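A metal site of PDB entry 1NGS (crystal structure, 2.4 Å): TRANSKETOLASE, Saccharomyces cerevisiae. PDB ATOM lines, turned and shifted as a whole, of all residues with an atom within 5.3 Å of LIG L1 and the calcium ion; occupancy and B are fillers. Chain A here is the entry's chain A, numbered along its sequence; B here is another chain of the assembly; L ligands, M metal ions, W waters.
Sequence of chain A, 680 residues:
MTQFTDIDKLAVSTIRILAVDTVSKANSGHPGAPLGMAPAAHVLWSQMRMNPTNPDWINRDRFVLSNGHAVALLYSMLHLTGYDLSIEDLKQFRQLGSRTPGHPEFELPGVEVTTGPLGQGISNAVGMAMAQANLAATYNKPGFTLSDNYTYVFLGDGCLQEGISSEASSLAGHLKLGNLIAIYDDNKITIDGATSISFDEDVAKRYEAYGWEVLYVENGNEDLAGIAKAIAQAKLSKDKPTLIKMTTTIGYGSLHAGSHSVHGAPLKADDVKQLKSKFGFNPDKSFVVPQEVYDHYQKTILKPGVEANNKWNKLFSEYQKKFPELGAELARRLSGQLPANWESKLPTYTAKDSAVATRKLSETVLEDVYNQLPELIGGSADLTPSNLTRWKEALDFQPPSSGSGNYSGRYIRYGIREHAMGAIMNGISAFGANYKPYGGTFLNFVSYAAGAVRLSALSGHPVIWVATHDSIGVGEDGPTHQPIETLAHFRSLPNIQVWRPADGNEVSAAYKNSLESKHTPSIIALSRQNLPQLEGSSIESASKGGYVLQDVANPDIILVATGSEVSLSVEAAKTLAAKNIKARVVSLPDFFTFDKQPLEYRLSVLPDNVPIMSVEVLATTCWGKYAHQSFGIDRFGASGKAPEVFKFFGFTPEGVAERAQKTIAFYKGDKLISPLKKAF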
ATOM      1  N   ALA A  33       6.732  -7.124  33.005  1.00  0.00           N
ATOM      2  CA  ALA A  33       5.630  -6.178  33.178  1.00  0.00           C
ATOM      3  C   ALA A  33       5.408  -5.797  34.641  1.00  0.00           C
ATOM      4  O   ALA A  33       5.173  -4.630  34.938  1.00  0.00           O
ATOM      5  CB  ALA A  33       4.355  -6.705  32.547  1.00  0.00           C
ATOM      6  N   ASN A  67      -3.533  -7.834  30.684  1.00  0.00           N
ATOM      7  CA  ASN A  67      -2.272  -8.536  30.411  1.00  0.00           C
ATOM      8  C   ASN A  67      -2.006  -9.506  31.570  1.00  0.00           C
ATOM      9  O   ASN A  67      -1.063  -9.346  32.348  1.00  0.00           O
ATOM     10  CB  ASN A  67      -1.121  -7.546  30.237  1.00  0.00           C
ATOM     11  CG  ASN A  67      -1.063  -6.453  31.310  1.00  0.00           C
ATOM     12  OD1 ASN A  67      -0.062  -5.750  31.404  1.00  0.00           O
ATOM     13  ND2 ASN A  67      -2.134  -6.281  32.083  1.00  0.00           N
ATOM     14  N   HIS A  69      -0.513 -12.290  32.122  1.00  0.00           N
ATOM     15  CA  HIS A  69       0.792 -12.868  32.398  1.00  0.00           C
ATOM     16  C   HIS A  69       1.504 -12.141  33.527  1.00  0.00           C
ATOM     17  O   HIS A  69       2.364 -12.722  34.215  1.00  0.00           O
ATOM     18  CB  HIS A  69       1.655 -12.985  31.123  1.00  0.00           C
ATOM     19  CG  HIS A  69       1.940 -11.673  30.425  1.00  0.00           C
ATOM     20  ND1 HIS A  69       1.180 -11.224  29.370  1.00  0.00           N
ATOM     21  CD2 HIS A  69       2.917 -10.766  30.615  1.00  0.00           C
ATOM     22  CE1 HIS A  69       1.685 -10.076  28.935  1.00  0.00           C
ATOM     23  NE2 HIS A  69       2.740  -9.777  29.675  1.00  0.00           N
ATOM     24  N   GLY A 116      -5.464 -14.417  30.589  1.00  0.00           N
ATOM     25  CA  GLY A 116      -4.317 -15.205  30.196  1.00  0.00           C
ATOM     26  C   GLY A 116      -4.375 -14.951  28.712  1.00  0.00           C
ATOM     27  O   GLY A 116      -3.399 -14.469  28.139  1.00  0.00           O
ATOM     28  N   PRO A 117      -5.503 -15.301  28.050  1.00  0.00           N
ATOM     29  CA  PRO A 117      -5.695 -15.088  26.612  1.00  0.00           C
ATOM     30  C   PRO A 117      -5.721 -13.567  26.411  1.00  0.00           C
ATOM     31  O   PRO A 117      -6.523 -12.856  27.057  1.00  0.00           O
ATOM     32  CB  PRO A 117      -7.092 -15.669  26.371  1.00  0.00           C
ATOM     33  CG  PRO A 117      -7.188 -16.754  27.353  1.00  0.00           C
ATOM     34  CD  PRO A 117      -6.592 -16.142  28.597  1.00  0.00           C
ATOM     35  N   LEU A 118      -4.844 -13.072  25.554  1.00  0.00           N
ATOM     36  CA  LEU A 118      -4.779 -11.636  25.324  1.00  0.00           C
ATOM     37  C   LEU A 118      -6.031 -11.117  24.643  1.00  0.00           C
ATOM     38  O   LEU A 118      -6.700 -11.824  23.894  1.00  0.00           O
ATOM     39  CB  LEU A 118      -3.551 -11.273  24.493  1.00  0.00           C
ATOM     40  CG  LEU A 118      -2.215 -11.559  25.176  1.00  0.00           C
ATOM     41  CD1 LEU A 118      -1.025 -11.129  24.317  1.00  0.00           C
ATOM     42  CD2 LEU A 118      -2.222 -10.812  26.473  1.00  0.00           C
ATOM     43  N   GLY A 156      -1.354  -4.375  27.593  1.00  0.00           N
ATOM     44  CA  GLY A 156      -0.091  -4.302  26.899  1.00  0.00           C
ATOM     45  C   GLY A 156      -0.227  -4.274  25.394  1.00  0.00           C
ATOM     46  O   GLY A 156      -1.337  -4.218  24.852  1.00  0.00           O
ATOM     47  N   ASP A 157       0.901  -4.364  24.711  1.00  0.00           N
ATOM     48  CA  ASP A 157       0.876  -4.340  23.257  1.00  0.00           C
ATOM     49  C   ASP A 157       0.110  -5.543  22.701  1.00  0.00           C
ATOM     50  O   ASP A 157      -0.625  -5.409  21.716  1.00  0.00           O
ATOM     51  CB  ASP A 157       2.300  -4.216  22.719  1.00  0.00           C
ATOM     52  CG  ASP A 157       3.080  -3.093  23.375  1.00  0.00           C
ATOM     53  OD1 ASP A 157       3.707  -3.318  24.422  1.00  0.00           O
ATOM     54  OD2 ASP A 157       3.044  -1.976  22.832  1.00  0.00           O
ATOM     55  N   GLY A 158       0.200  -6.688  23.379  1.00  0.00           N
ATOM     56  CA  GLY A 158      -0.499  -7.884  22.933  1.00  0.00           C
ATOM     57  C   GLY A 158      -2.001  -7.710  22.890  1.00  0.00           C
ATOM     58  O   GLY A 158      -2.647  -8.137  21.935  1.00  0.00           O
ATOM     59  N   CYS A 159      -2.557  -7.102  23.942  1.00  0.00           N
ATOM     60  CA  CYS A 159      -3.999  -6.857  24.010  1.00  0.00           C
ATOM     61  C   CYS A 159      -4.453  -5.920  22.885  1.00  0.00           C
ATOM     62  O   CYS A 159      -5.514  -6.111  22.313  1.00  0.00           O
ATOM     63  CB  CYS A 159      -4.400  -6.283  25.379  1.00  0.00           C
ATOM     64  SG  CYS A 159      -4.331  -7.472  26.738  1.00  0.00           S
ATOM     65  N   GLU A 162      -4.747  -7.833  19.284  1.00  0.00           N
ATOM     66  CA  GLU A 162      -5.857  -8.763  19.097  1.00  0.00           C
ATOM     67  C   GLU A 162      -7.139  -8.054  18.654  1.00  0.00           C
ATOM     68  O   GLU A 162      -7.631  -7.141  19.335  1.00  0.00           O
ATOM     69  CB  GLU A 162      -6.107  -9.561  20.386  1.00  0.00           C
ATOM     70  CG  GLU A 162      -4.993 -10.557  20.734  1.00  0.00           C
ATOM     71  CD  GLU A 162      -5.124 -11.862  19.970  1.00  0.00           C
ATOM     72  OE1 GLU A 162      -5.773 -11.885  18.914  1.00  0.00           O
ATOM     73  OE2 GLU A 162      -4.611 -12.880  20.461  1.00  0.00           O
ATOM     74  N   ASP A 185       0.538  -0.171  29.053  1.00  0.00           N
ATOM     75  CA  ASP A 185       1.949  -0.428  29.299  1.00  0.00           C
ATOM     76  C   ASP A 185       2.692  -0.346  27.969  1.00  0.00           C
ATOM     77  O   ASP A 185       2.853  -1.341  27.258  1.00  0.00           O
ATOM     78  CB  ASP A 185       2.120  -1.833  29.918  1.00  0.00           C
ATOM     79  CG  ASP A 185       3.506  -2.069  30.494  1.00  0.00           C
ATOM     80  OD1 ASP A 185       4.274  -1.103  30.676  1.00  0.00           O
ATOM     81  OD2 ASP A 185       3.832  -3.245  30.772  1.00  0.00           O
ATOM     82  N   ASN A 187       5.724  -0.372  26.585  1.00  0.00           N
ATOM     83  CA  ASN A 187       7.120  -0.693  26.818  1.00  0.00           C
ATOM     84  C   ASN A 187       7.990  -1.076  25.627  1.00  0.00           C
ATOM     85  O   ASN A 187       9.192  -1.318  25.800  1.00  0.00           O
ATOM     86  CB  ASN A 187       7.269  -1.725  27.935  1.00  0.00           C
ATOM     87  CG  ASN A 187       6.610  -3.049  27.617  1.00  0.00           C
ATOM     88  OD1 ASN A 187       6.190  -3.284  26.477  1.00  0.00           O
ATOM     89  ND2 ASN A 187       6.523  -3.925  28.613  1.00  0.00           N
ATOM     90  N   LYS A 188       7.397  -1.138  24.445  1.00  0.00           N
ATOM     91  CA  LYS A 188       8.122  -1.436  23.204  1.00  0.00           C
ATOM     92  C   LYS A 188       8.646  -2.864  23.030  1.00  0.00           C
ATOM     93  O   LYS A 188       9.465  -3.119  22.136  1.00  0.00           O
ATOM     94  CB  LYS A 188       9.282  -0.452  23.021  1.00  0.00           C
ATOM     95  CG  LYS A 188       8.903   0.956  22.532  1.00  0.00           C
ATOM     96  CD  LYS A 188       8.311   1.909  23.601  1.00  0.00           C
ATOM     97  CE  LYS A 188       8.264   3.352  23.058  1.00  0.00           C
ATOM     98  NZ  LYS A 188       7.077   4.188  23.445  1.00  0.00           N
ATOM     99  N   ILE A 189       8.153  -3.795  23.832  1.00  0.00           N
ATOM    100  CA  ILE A 189       8.626  -5.177  23.774  1.00  0.00           C
ATOM    101  C   ILE A 189       7.477  -6.158  23.845  1.00  0.00           C
ATOM    102  O   ILE A 189       6.448  -5.880  24.444  1.00  0.00           O
ATOM    103  CB  ILE A 189       9.605  -5.461  24.969  1.00  0.00           C
ATOM    104  CG1 ILE A 189      11.028  -4.968  24.637  1.00  0.00           C
ATOM    105  CG2 ILE A 189       9.592  -6.940  25.396  1.00  0.00           C
ATOM    106  CD1 ILE A 189      11.825  -5.906  23.768  1.00  0.00           C
ATOM    107  N   THR A 190       7.625  -7.255  23.106  1.00  0.00           N
ATOM    108  CA  THR A 190       6.677  -8.356  23.122  1.00  0.00           C
ATOM    109  C   THR A 190       7.591  -9.579  23.024  1.00  0.00           C
ATOM    110  O   THR A 190       8.818  -9.424  22.996  1.00  0.00           O
ATOM    111  CB  THR A 190       5.650  -8.299  21.954  1.00  0.00           C
ATOM    112  OG1 THR A 190       6.310  -8.419  20.690  1.00  0.00           O
ATOM    113  CG2 THR A 190       4.874  -6.991  22.001  1.00  0.00           C
ATOM    114  N   ILE A 191       7.035 -10.779  22.972  1.00  0.00           N
ATOM    115  CA  ILE A 191       7.852 -11.985  22.902  1.00  0.00           C
ATOM    116  C   ILE A 191       8.907 -12.038  21.771  1.00  0.00           C
ATOM    117  O   ILE A 191      10.094 -12.234  22.049  1.00  0.00           O
ATOM    118  CB  ILE A 191       6.944 -13.236  22.876  1.00  0.00           C
ATOM    119  CG1 ILE A 191       6.215 -13.372  24.213  1.00  0.00           C
ATOM    120  CG2 ILE A 191       7.743 -14.486  22.550  1.00  0.00           C
ATOM    121  CD1 ILE A 191       5.296 -14.536  24.257  1.00  0.00           C
ATOM    122  N   ILE A 250      10.344  -2.415  30.283  1.00  0.00           N
ATOM    123  CA  ILE A 250      10.097  -3.798  30.697  1.00  0.00           C
ATOM    124  C   ILE A 250      11.263  -4.238  31.580  1.00  0.00           C
ATOM    125  O   ILE A 250      12.414  -3.978  31.247  1.00  0.00           O
ATOM    126  CB  ILE A 250       9.931  -4.762  29.457  1.00  0.00           C
ATOM    127  CG1 ILE A 250       9.299  -6.080  29.884  1.00  0.00           C
ATOM    128  CG2 ILE A 250      11.274  -5.057  28.770  1.00  0.00           C
ATOM    129  CD1 ILE A 250       8.953  -6.945  28.722  1.00  0.00           C
ATOM    130  N   HIS A 263      10.873 -10.775  29.577  1.00  0.00           N
ATOM    131  CA  HIS A 263       9.429 -10.925  29.423  1.00  0.00           C
ATOM    132  C   HIS A 263       8.858 -12.123  30.167  1.00  0.00           C
ATOM    133  O   HIS A 263       7.951 -11.964  30.992  1.00  0.00           O
ATOM    134  CB  HIS A 263       8.963 -10.972  27.947  1.00  0.00           C
ATOM    135  CG  HIS A 263       7.663 -11.715  27.746  1.00  0.00           C
ATOM    136  ND1 HIS A 263       6.431 -11.191  28.062  1.00  0.00           N
ATOM    137  CD2 HIS A 263       7.432 -12.984  27.340  1.00  0.00           C
ATOM    138  CE1 HIS A 263       5.503 -12.093  27.872  1.00  0.00           C
ATOM    139  NE2 HIS A 263       6.078 -13.206  27.427  1.00  0.00           N
ATOM    140  N   ALA B 381       2.870 -15.984  15.325  1.00  0.00           N
ATOM    141  CA  ALA B 381       2.075 -14.906  15.905  1.00  0.00           C
ATOM    142  C   ALA B 381       2.719 -14.547  17.251  1.00  0.00           C
ATOM    143  O   ALA B 381       2.182 -14.886  18.311  1.00  0.00           O
ATOM    144  CB  ALA B 381       0.622 -15.347  16.120  1.00  0.00           C
ATOM    145  N   ASP B 382       3.883 -13.907  17.182  1.00  0.00           N
ATOM    146  CA  ASP B 382       4.652 -13.484  18.340  1.00  0.00           C
ATOM    147  C   ASP B 382       5.100 -14.606  19.287  1.00  0.00           C
ATOM    148  O   ASP B 382       5.186 -14.391  20.490  1.00  0.00           O
ATOM    149  CB  ASP B 382       3.913 -12.402  19.141  1.00  0.00           C
ATOM    150  CG  ASP B 382       4.849 -11.521  19.958  1.00  0.00           C
ATOM    151  OD1 ASP B 382       5.829 -10.991  19.419  1.00  0.00           O
ATOM    152  OD2 ASP B 382       4.629 -11.363  21.168  1.00  0.00           O
ATOM    153  N   LEU B 383       5.437 -15.773  18.748  1.00  0.00           N
ATOM    154  CA  LEU B 383       5.874 -16.888  19.594  1.00  0.00           C
ATOM    155  C   LEU B 383       7.014 -17.678  18.968  1.00  0.00           C
ATOM    156  O   LEU B 383       7.237 -18.845  19.276  1.00  0.00           O
ATOM    157  CB  LEU B 383       4.716 -17.836  19.883  1.00  0.00           C
ATOM    158  CG  LEU B 383       3.716 -17.466  20.984  1.00  0.00           C
ATOM    159  CD1 LEU B 383       2.512 -18.388  20.876  1.00  0.00           C
ATOM    160  CD2 LEU B 383       4.365 -17.558  22.357  1.00  0.00           C
ATOM    161  N   ILE B 416       0.623 -10.556  17.666  1.00  0.00           N
ATOM    162  CA  ILE B 416      -0.407 -11.320  18.365  1.00  0.00           C
ATOM    163  C   ILE B 416      -1.695 -11.126  17.553  1.00  0.00           C
ATOM    164  O   ILE B 416      -2.551 -10.313  17.894  1.00  0.00           O
ATOM    165  CB  ILE B 416      -0.561 -10.826  19.845  1.00  0.00           C
ATOM    166  CG1 ILE B 416       0.731 -11.037  20.629  1.00  0.00           C
ATOM    167  CG2 ILE B 416      -1.608 -11.636  20.560  1.00  0.00           C
ATOM    168  CD1 ILE B 416       1.723  -9.916  20.510  1.00  0.00           C
ATOM    169  N   GLU B 418      -3.690 -14.066  15.743  1.00  0.00           N
ATOM    170  CA  GLU B 418      -3.954 -15.420  15.257  1.00  0.00           C
ATOM    171  C   GLU B 418      -4.971 -15.554  14.124  1.00  0.00           C
ATOM    172  O   GLU B 418      -4.705 -16.225  13.119  1.00  0.00           O
ATOM    173  CB  GLU B 418      -4.303 -16.335  16.439  1.00  0.00           C
ATOM    174  CG  GLU B 418      -3.121 -16.546  17.425  1.00  0.00           C
ATOM    175  CD  GLU B 418      -3.109 -15.555  18.590  1.00  0.00           C
ATOM    176  OE1 GLU B 418      -4.077 -14.811  18.768  1.00  0.00           O
ATOM    177  OE2 GLU B 418      -2.125 -15.542  19.346  1.00  0.00           O
ATOM    178  N   PHE B 442       0.233 -21.282  19.906  1.00  0.00           N
ATOM    179  CA  PHE B 442      -0.011 -22.363  20.858  1.00  0.00           C
ATOM    180  C   PHE B 442      -1.334 -23.000  20.432  1.00  0.00           C
ATOM    181  O   PHE B 442      -2.275 -22.277  20.099  1.00  0.00           O
ATOM    182  CB  PHE B 442      -0.162 -21.795  22.278  1.00  0.00           C
ATOM    183  CG  PHE B 442       1.121 -21.274  22.899  1.00  0.00           C
ATOM    184  CD1 PHE B 442       2.371 -21.759  22.508  1.00  0.00           C
ATOM    185  CD2 PHE B 442       1.073 -20.323  23.919  1.00  0.00           C
ATOM    186  CE1 PHE B 442       3.544 -21.322  23.140  1.00  0.00           C
ATOM    187  CE2 PHE B 442       2.246 -19.886  24.551  1.00  0.00           C
ATOM    188  CZ  PHE B 442       3.477 -20.382  24.161  1.00  0.00           C
ATOM    189  N   PHE B 445      -4.661 -21.448  21.171  1.00  0.00           N
ATOM    190  CA  PHE B 445      -5.016 -20.189  20.560  1.00  0.00           C
ATOM    191  C   PHE B 445      -5.326 -20.251  19.075  1.00  0.00           C
ATOM    192  O   PHE B 445      -5.667 -19.239  18.454  1.00  0.00           O
ATOM    193  CB  PHE B 445      -3.998 -19.149  20.975  1.00  0.00           C
ATOM    194  CG  PHE B 445      -3.924 -18.973  22.474  1.00  0.00           C
ATOM    195  CD1 PHE B 445      -5.086 -18.854  23.224  1.00  0.00           C
ATOM    196  CD2 PHE B 445      -2.697 -18.922  23.125  1.00  0.00           C
ATOM    197  CE1 PHE B 445      -5.045 -18.708  24.597  1.00  0.00           C
ATOM    198  CE2 PHE B 445      -2.642 -18.772  24.507  1.00  0.00           C
ATOM    199  CZ  PHE B 445      -3.818 -18.658  25.247  1.00  0.00           C
ATOM    200  N   TYR B 448      -8.747 -19.031  18.395  1.00  0.00           N
ATOM    201  CA  TYR B 448      -9.003 -17.622  18.147  1.00  0.00           C
ATOM    202  C   TYR B 448      -9.194 -17.416  16.650  1.00  0.00           C
ATOM    203  O   TYR B 448      -9.852 -16.455  16.217  1.00  0.00           O
ATOM    204  CB  TYR B 448      -7.797 -16.792  18.579  1.00  0.00           C
ATOM    205  CG  TYR B 448      -7.920 -16.132  19.927  1.00  0.00           C
ATOM    206  CD1 TYR B 448      -8.169 -16.887  21.090  1.00  0.00           C
ATOM    207  CD2 TYR B 448      -7.757 -14.759  20.058  1.00  0.00           C
ATOM    208  CE1 TYR B 448      -8.250 -16.268  22.322  1.00  0.00           C
ATOM    209  CE2 TYR B 448      -7.830 -14.147  21.281  1.00  0.00           C
ATOM    210  CZ  TYR B 448      -8.082 -14.893  22.402  1.00  0.00           C
ATOM    211  OH  TYR B 448      -8.161 -14.220  23.598  1.00  0.00           O
ATOM    212  N   HIS B 481      -4.254 -21.850  29.214  1.00  0.00           N
ATOM    213  CA  HIS B 481      -3.366 -22.212  28.101  1.00  0.00           C
ATOM    214  C   HIS B 481      -3.341 -23.645  27.656  1.00  0.00           C
ATOM    215  O   HIS B 481      -2.830 -23.945  26.576  1.00  0.00           O
ATOM    216  CB  HIS B 481      -1.929 -21.828  28.387  1.00  0.00           C
ATOM    217  CG  HIS B 481      -1.693 -20.348  28.414  1.00  0.00           C
ATOM    218  ND1 HIS B 481      -2.513 -19.490  29.102  1.00  0.00           N
ATOM    219  CD2 HIS B 481      -0.737 -19.593  27.847  1.00  0.00           C
ATOM    220  CE1 HIS B 481      -2.072 -18.255  28.948  1.00  0.00           C
ATOM    221  NE2 HIS B 481      -0.996 -18.285  28.197  1.00  0.00           N
HETATM  222  N1  LIG L   1      -2.148 -14.921  22.120  1.00  0.00           N
HETATM  223  C1  LIG L   1      -3.142 -15.007  23.017  1.00  0.00           C
HETATM  224  C2  LIG L   1      -4.514 -14.850  22.542  1.00  0.00           C
HETATM  225  N2  LIG L   1      -2.899 -15.274  24.280  1.00  0.00           N
HETATM  226  C3  LIG L   1      -1.591 -15.406  24.731  1.00  0.00           C
HETATM  227  N3  LIG L   1      -1.455 -15.709  26.029  1.00  0.00           N
HETATM  228  C4  LIG L   1      -0.502 -15.359  23.809  1.00  0.00           C
HETATM  229  C5  LIG L   1      -0.845 -15.104  22.517  1.00  0.00           C
HETATM  230  C6  LIG L   1       0.920 -15.712  24.198  1.00  0.00           C
HETATM  231  N4  LIG L   1       1.587 -14.504  24.864  1.00  0.00           N
HETATM  232  C7  LIG L   1       1.592 -14.214  26.178  1.00  0.00           C
HETATM  233  S1  LIG L   1       2.191 -12.659  26.528  1.00  0.00           S
HETATM  234  C8  LIG L   1       2.509 -12.447  24.879  1.00  0.00           C
HETATM  235  C9  LIG L   1       2.153 -13.558  24.161  1.00  0.00           C
HETATM  236  C10 LIG L   1       2.363 -13.762  22.726  1.00  0.00           C
HETATM  237  C11 LIG L   1       3.145 -11.188  24.369  1.00  0.00           C
HETATM  238  C12 LIG L   1       3.420 -10.187  25.413  1.00  0.00           C
HETATM  239  O1  LIG L   1       2.945  -8.963  24.866  1.00  0.00           O
HETATM  240  P1  LIG L   1       2.515  -7.870  25.868  1.00  0.00           P
HETATM  241  O2  LIG L   1       1.035  -7.665  26.092  1.00  0.00           O
HETATM  242  O3  LIG L   1       3.262  -6.790  25.250  1.00  0.00           O
HETATM  243  O4  LIG L   1       3.439  -7.998  27.185  1.00  0.00           O
HETATM  244  P2  LIG L   1       4.918  -7.793  27.776  1.00  0.00           P
HETATM  245  O5  LIG L   1       4.872  -6.326  27.713  1.00  0.00           O
HETATM  246  O6  LIG L   1       4.842  -8.296  29.159  1.00  0.00           O
HETATM  247  O7  LIG L   1       5.901  -8.556  26.955  1.00  0.00           O
HETATM  248  C1  LG2 L   2       4.848 -16.054  28.004  1.00  0.00           C
HETATM  249  O1  LG2 L   2       3.961 -15.193  27.905  1.00  0.00           O
HETATM  250  C2  LG2 L   2       4.536 -17.538  27.847  1.00  0.00           C
HETATM  251  O2  LG2 L   2       3.276 -17.883  28.473  1.00  0.00           O
HETATM  252  C3  LG2 L   2       5.661 -18.323  28.511  1.00  0.00           C
HETATM  253  O3  LG2 L   2       6.787 -17.452  28.776  1.00  0.00           O
HETATM  254  C4  LG2 L   2       6.115 -19.391  27.547  1.00  0.00           C
HETATM  255  O4  LG2 L   2       7.087 -20.171  28.240  1.00  0.00           O
HETATM  256  P1  LG2 L   2       7.625 -21.243  27.377  1.00  0.00           P
HETATM  257  O5  LG2 L   2       9.028 -21.740  27.945  1.00  0.00           O
HETATM  258  O6  LG2 L   2       7.812 -20.666  25.904  1.00  0.00           O
HETATM  259  O7  LG2 L   2       6.586 -22.458  27.357  1.00  0.00           O
HETATM  260 CA    CA M   1       4.715  -4.821  25.589  1.00  0.00          CA
HETATM  261  O   HOH W   1      -1.646  -7.413  26.864  1.00  0.00           O
HETATM  262  O   HOH W   2       0.531 -15.740  28.968  1.00  0.00           O
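The calcium ion is bound by the side-chain carboxylate of Asp 157 (2.2 Å), the side-chain amide oxygen of Asn 187 (2.3 Å), the backbone carbonyl oxygen of Ile 189 (2.3 Å), an oxygen (O3) of LIG L1 (2.5 Å) and an oxygen (O5) of LIG L1 (2.6 Å).
Water W1 lies within hydrogen-bond range of SG of Cys 159 (2.7 Å), O2 of LIG L1 (2.8 Å) and N of Gly 156 (3.1 Å).
O3 of LIG L1 lies close to N of Asp 157 (3.4 Å). O6 of LIG L1 lies within hydrogen-bond range of NE2 of His 69, 2.6 Å away. OE2 of Glu 418 of chain B is in hydrogen-bond range of N1 of LIG L1 (2.8 Å). O7 of LIG L1 lies within hydrogen-bond range of ND1 of His 263 (2.9 Å). The backbone NH of Gly 158 sits at hydrogen-bond distance from an oxygen (O2) of LIG L1 (3.0 Å). The backbone carbonyl oxygen (O) of Gly 116 sits at hydrogen-bond distance from a nitrogen (N3) of LIG L1 (3.1 Å). N of Leu 118 lies within hydrogen-bond range of N2 of LIG L1, at 3.2 Å. A nitrogen (N3) of LIG L1 sits at hydrogen-bond distance from a ring nitrogen (NE2) of His 481 of chain B, at 3.4 Å. A ring nitrogen (NE2) of His 263 lies within hydrogen-bond range of an oxygen (O1) of LG2 L2 (2.9 Å).
Merely in contact with LIG L1: Glu 162 (2.9 Å), Ile 191 (3.3 Å), Phe 445 of chain B (3.5 Å), Asp 382 of chain B (3.5 Å), Tyr 448 of chain B (3.6 Å), Thr 190 (3.6 Å), Gly 156 (3.6 Å), Pro 117 (3.6 Å), Ile 416 of chain B (3.7 Å), Ala 33 (3.8 Å) and Ile 250 (3.9 Å). Hydrophobic or aromatic side chains that line LIG L1: Ala 33, His 69, Leu 118, Ile 191, Ile 250, His 263, Ile 416 of chain B, Phe 445 of chain B, Tyr 448 of chain B and His 481 of chain B. Within 4 Å of LIG L1: Ala 33, His 69, Gly 116, Pro 117, Leu 118, Gly 156, Asp 157, Gly 158, Glu 162, Asn 187, Ile 189, Thr 190, Ile 191, Ile 250, His 263, Asp 382 of chain B, Ile 416 of chain B, Glu 418 of chain B, Phe 445 of chain B, Tyr 448 of chain B and His 481 of chain B. The nearest printed residue that does not touch LIG L1 is Cys 159 (4.2 Å).
OE1 of Glu 418 of chain B lies close to OE2 of Glu 162, at 2.6 Å. The backbone carbonyl oxygen of Leu 118 is in hydrogen-bond range of the side-chain hydroxyl of Tyr 448 of chain B (2.8 Å). The side-chain carboxylate (OD2) of Asp 382 of chain B sits at hydrogen-bond distance from the backbone NH (N) of Ile 191 (3.1 Å). OD1 of Asp 382 of chain B sits at hydrogen-bond distance from OG1 of Thr 190, at 2.9 Å.
Three residues have an atom within 4 Å of the calcium ion: Asp 157, Asn 187 and Ile 189.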
